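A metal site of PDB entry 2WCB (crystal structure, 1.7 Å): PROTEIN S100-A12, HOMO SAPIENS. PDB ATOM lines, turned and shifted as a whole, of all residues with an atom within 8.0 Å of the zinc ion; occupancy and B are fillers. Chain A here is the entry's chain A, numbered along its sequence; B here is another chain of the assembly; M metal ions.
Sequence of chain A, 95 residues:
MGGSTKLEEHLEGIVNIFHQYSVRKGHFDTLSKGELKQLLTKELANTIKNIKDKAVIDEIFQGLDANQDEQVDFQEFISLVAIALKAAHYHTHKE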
ATOM      1  N   VAL A  15      -3.411 -28.309  17.713  1.00  0.00           N
ATOM      2  CA  VAL A  15      -4.450 -27.984  18.710  1.00  0.00           C
ATOM      3  C   VAL A  15      -5.808 -28.511  18.348  1.00  0.00           C
ATOM      4  O   VAL A  15      -6.530 -29.078  19.203  1.00  0.00           O
ATOM      5  CB  VAL A  15      -4.601 -26.461  18.970  1.00  0.00           C
ATOM      6  CG1 VAL A  15      -5.835 -26.195  19.863  1.00  0.00           C
ATOM      7  CG2 VAL A  15      -3.346 -25.894  19.584  1.00  0.00           C
ATOM      8  N   PHE A  18      -5.832 -32.394  18.956  1.00  0.00           N
ATOM      9  CA  PHE A  18      -6.018 -32.610  20.379  1.00  0.00           C
ATOM     10  C   PHE A  18      -7.477 -32.455  20.782  1.00  0.00           C
ATOM     11  O   PHE A  18      -8.053 -33.342  21.448  1.00  0.00           O
ATOM     12  CB  PHE A  18      -5.138 -31.641  21.205  1.00  0.00           C
ATOM     13  CG  PHE A  18      -5.360 -31.737  22.715  1.00  0.00           C
ATOM     14  CD1 PHE A  18      -4.717 -32.714  23.477  1.00  0.00           C
ATOM     15  CD2 PHE A  18      -6.222 -30.850  23.369  1.00  0.00           C
ATOM     16  CE1 PHE A  18      -4.952 -32.793  24.898  1.00  0.00           C
ATOM     17  CE2 PHE A  18      -6.458 -30.933  24.762  1.00  0.00           C
ATOM     18  CZ  PHE A  18      -5.808 -31.882  25.534  1.00  0.00           C
ATOM     19  N   HIS A  19      -8.095 -31.362  20.337  1.00  0.00           N
ATOM     20  CA  HIS A  19      -9.469 -31.077  20.674  1.00  0.00           C
ATOM     21  C   HIS A  19     -10.475 -32.087  20.201  1.00  0.00           C
ATOM     22  O   HIS A  19     -11.470 -32.316  20.876  1.00  0.00           O
ATOM     23  CB  HIS A  19      -9.873 -29.692  20.214  1.00  0.00           C
ATOM     24  CG  HIS A  19      -9.358 -28.645  21.143  1.00  0.00           C
ATOM     25  ND1 HIS A  19      -9.107 -27.347  20.766  1.00  0.00           N
ATOM     26  CD2 HIS A  19      -9.007 -28.740  22.449  1.00  0.00           C
ATOM     27  CE1 HIS A  19      -8.664 -26.669  21.809  1.00  0.00           C
ATOM     28  NE2 HIS A  19      -8.610 -27.489  22.855  1.00  0.00           N
ATOM     29  N   SER A  22     -10.073 -34.534  23.041  1.00  0.00           N
ATOM     30  CA  SER A  22     -10.393 -34.031  24.376  1.00  0.00           C
ATOM     31  C   SER A  22     -11.916 -33.740  24.577  1.00  0.00           C
ATOM     32  O   SER A  22     -12.432 -33.968  25.680  1.00  0.00           O
ATOM     33  CB  SER A  22      -9.536 -32.806  24.684  1.00  0.00           C
ATOM     34  OG  SER A  22      -9.963 -31.693  23.948  1.00  0.00           O
ATOM     35  N   VAL A  23     -12.637 -33.301  23.542  1.00  0.00           N
ATOM     36  CA  VAL A  23     -14.034 -32.922  23.705  1.00  0.00           C
ATOM     37  C   VAL A  23     -14.978 -34.097  23.856  1.00  0.00           C
ATOM     38  O   VAL A  23     -16.119 -33.899  24.279  1.00  0.00           O
ATOM     39  CB  VAL A  23     -14.602 -32.076  22.550  1.00  0.00           C
ATOM     40  CG1 VAL A  23     -13.824 -30.777  22.414  1.00  0.00           C
ATOM     41  CG2 VAL A  23     -14.720 -32.901  21.251  1.00  0.00           C
ATOM     42  N   PHE A  28     -14.000 -30.859  28.350  1.00  0.00           N
ATOM     43  CA  PHE A  28     -13.605 -30.761  26.925  1.00  0.00           C
ATOM     44  C   PHE A  28     -12.114 -30.543  26.672  1.00  0.00           C
ATOM     45  O   PHE A  28     -11.684 -30.725  25.553  1.00  0.00           O
ATOM     46  CB  PHE A  28     -14.442 -29.738  26.105  1.00  0.00           C
ATOM     47  CG  PHE A  28     -14.121 -28.306  26.387  1.00  0.00           C
ATOM     48  CD1 PHE A  28     -12.861 -27.808  26.144  1.00  0.00           C
ATOM     49  CD2 PHE A  28     -15.099 -27.458  26.869  1.00  0.00           C
ATOM     50  CE1 PHE A  28     -12.580 -26.500  26.419  1.00  0.00           C
ATOM     51  CE2 PHE A  28     -14.825 -26.142  27.135  1.00  0.00           C
ATOM     52  CZ  PHE A  28     -13.549 -25.658  26.923  1.00  0.00           C
ATOM     53  N   ASP A  29     -11.351 -30.162  27.686  1.00  0.00           N
ATOM     54  CA  ASP A  29      -9.922 -29.849  27.511  1.00  0.00           C
ATOM     55  C   ASP A  29      -8.902 -30.831  28.100  1.00  0.00           C
ATOM     56  O   ASP A  29      -7.704 -30.503  28.145  1.00  0.00           O
ATOM     57  CB  ASP A  29      -9.613 -28.470  28.060  1.00  0.00           C
ATOM     58  CG  ASP A  29      -8.793 -27.645  27.081  1.00  0.00           C
ATOM     59  OD1 ASP A  29      -8.892 -27.947  25.849  1.00  0.00           O
ATOM     60  OD2 ASP A  29      -8.048 -26.743  27.503  1.00  0.00           O
ATOM     61  N   THR A  30      -9.380 -31.981  28.581  1.00  0.00           N
ATOM     62  CA  THR A  30      -8.480 -33.055  29.021  1.00  0.00           C
ATOM     63  C   THR A  30      -8.951 -34.345  28.414  1.00  0.00           C
ATOM     64  O   THR A  30     -10.062 -34.430  27.888  1.00  0.00           O
ATOM     65  CB  THR A  30      -8.407 -33.202  30.568  1.00  0.00           C
ATOM     66  OG1 THR A  30      -9.674 -33.642  31.094  1.00  0.00           O
ATOM     67  CG2 THR A  30      -7.996 -31.892  31.250  1.00  0.00           C
ATOM     68  N   PHE A  74      -3.449 -30.610  27.843  1.00  0.00           N
ATOM     69  CA  PHE A  74      -2.729 -30.189  26.655  1.00  0.00           C
ATOM     70  C   PHE A  74      -1.193 -30.185  26.891  1.00  0.00           C
ATOM     71  O   PHE A  74      -0.418 -30.600  26.063  1.00  0.00           O
ATOM     72  CB  PHE A  74      -3.243 -28.847  26.130  1.00  0.00           C
ATOM     73  CG  PHE A  74      -2.720 -28.505  24.763  1.00  0.00           C
ATOM     74  CD1 PHE A  74      -3.142 -29.235  23.664  1.00  0.00           C
ATOM     75  CD2 PHE A  74      -1.772 -27.536  24.583  1.00  0.00           C
ATOM     76  CE1 PHE A  74      -2.668 -28.958  22.365  1.00  0.00           C
ATOM     77  CE2 PHE A  74      -1.265 -27.244  23.325  1.00  0.00           C
ATOM     78  CZ  PHE A  74      -1.710 -27.993  22.172  1.00  0.00           C
ATOM     79  N   ALA B  88      -0.595 -20.774  21.398  1.00  0.00           N
ATOM     80  CA  ALA B  88      -1.618 -20.945  20.413  1.00  0.00           C
ATOM     81  C   ALA B  88      -2.862 -21.666  21.010  1.00  0.00           C
ATOM     82  O   ALA B  88      -4.028 -21.352  20.624  1.00  0.00           O
ATOM     83  CB  ALA B  88      -1.089 -21.787  19.294  1.00  0.00           C
ATOM     84  N   HIS B  89      -2.638 -22.606  21.947  1.00  0.00           N
ATOM     85  CA  HIS B  89      -3.769 -23.326  22.579  1.00  0.00           C
ATOM     86  C   HIS B  89      -4.518 -22.329  23.393  1.00  0.00           C
ATOM     87  O   HIS B  89      -5.722 -22.129  23.313  1.00  0.00           O
ATOM     88  CB  HIS B  89      -3.300 -24.557  23.379  1.00  0.00           C
ATOM     89  CG  HIS B  89      -4.421 -25.263  24.109  1.00  0.00           C
ATOM     90  ND1 HIS B  89      -4.532 -25.258  25.465  1.00  0.00           N
ATOM     91  CD2 HIS B  89      -5.498 -25.965  23.647  1.00  0.00           C
ATOM     92  CE1 HIS B  89      -5.633 -25.889  25.844  1.00  0.00           C
ATOM     93  NE2 HIS B  89      -6.228 -26.353  24.758  1.00  0.00           N
ATOM     94  N   TYR B  90      -3.767 -21.610  24.169  1.00  0.00           N
ATOM     95  CA  TYR B  90      -4.403 -20.694  25.011  1.00  0.00           C
ATOM     96  C   TYR B  90      -5.277 -19.698  24.204  1.00  0.00           C
ATOM     97  O   TYR B  90      -6.411 -19.343  24.600  1.00  0.00           O
ATOM     98  CB  TYR B  90      -3.316 -19.989  25.760  1.00  0.00           C
ATOM     99  CG  TYR B  90      -3.884 -19.155  26.780  1.00  0.00           C
ATOM    100  CD1 TYR B  90      -4.478 -19.696  27.924  1.00  0.00           C
ATOM    101  CD2 TYR B  90      -3.871 -17.742  26.643  1.00  0.00           C
ATOM    102  CE1 TYR B  90      -5.032 -18.850  28.907  1.00  0.00           C
ATOM    103  CE2 TYR B  90      -4.413 -16.939  27.562  1.00  0.00           C
ATOM    104  CZ  TYR B  90      -4.993 -17.470  28.704  1.00  0.00           C
ATOM    105  OH  TYR B  90      -5.529 -16.560  29.611  1.00  0.00           O
ATOM    106  N   THR B  92      -6.816 -20.202  21.391  1.00  0.00           N
ATOM    107  CA  THR B  92      -8.067 -20.767  20.964  1.00  0.00           C
ATOM    108  C   THR B  92      -9.179 -20.697  22.004  1.00  0.00           C
ATOM    109  O   THR B  92     -10.324 -20.936  21.649  1.00  0.00           O
ATOM    110  CB  THR B  92      -7.864 -22.217  20.554  1.00  0.00           C
ATOM    111  OG1 THR B  92      -7.564 -22.975  21.753  1.00  0.00           O
ATOM    112  CG2 THR B  92      -6.716 -22.308  19.531  1.00  0.00           C
ATOM    113  N   HIS B  93      -8.872 -20.295  23.261  1.00  0.00           N
ATOM    114  CA  HIS B  93      -9.810 -20.302  24.357  1.00  0.00           C
ATOM    115  C   HIS B  93     -10.098 -18.898  24.805  1.00  0.00           C
ATOM    116  O   HIS B  93     -10.881 -18.724  25.675  1.00  0.00           O
ATOM    117  CB  HIS B  93      -9.265 -21.062  25.592  1.00  0.00           C
ATOM    118  CG  HIS B  93      -9.251 -22.545  25.368  1.00  0.00           C
ATOM    119  ND1 HIS B  93     -10.404 -23.281  25.371  1.00  0.00           N
ATOM    120  CD2 HIS B  93      -8.248 -23.388  25.078  1.00  0.00           C
ATOM    121  CE1 HIS B  93     -10.098 -24.550  25.044  1.00  0.00           C
ATOM    122  NE2 HIS B  93      -8.793 -24.626  24.872  1.00  0.00           N
HETATM  123 ZN    ZN M   1      -8.154 -26.510  24.621  1.00  0.00          ZN
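The backbone carbonyl oxygen (O) of His 89 of chain B is in hydrogen-bond range of the side-chain hydroxyl (OG1) of Thr 92 of chain B (2.6 Å). ND1 of His 19 lies close to O of Val 15. The side-chain hydroxyl of Ser 22 lies close to the backbone carbonyl oxygen of His 19, 3.5 Å away.
Four residues have an atom within 4 Å of the zinc ion: His 19, Asp 29, His 89 of chain B and His 93 of chain B. The nearest printed residue that does not touch the zinc ion is Thr 92 of chain B (4.6 Å).
The zinc ion is bound by NE2 of His 89 of chain B (1.9 Å), NE2 of His 93 of chain B (2.0 Å), OD1 of Asp 29 (2.0 Å) and NE2 of His 19 (2.1 Å).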
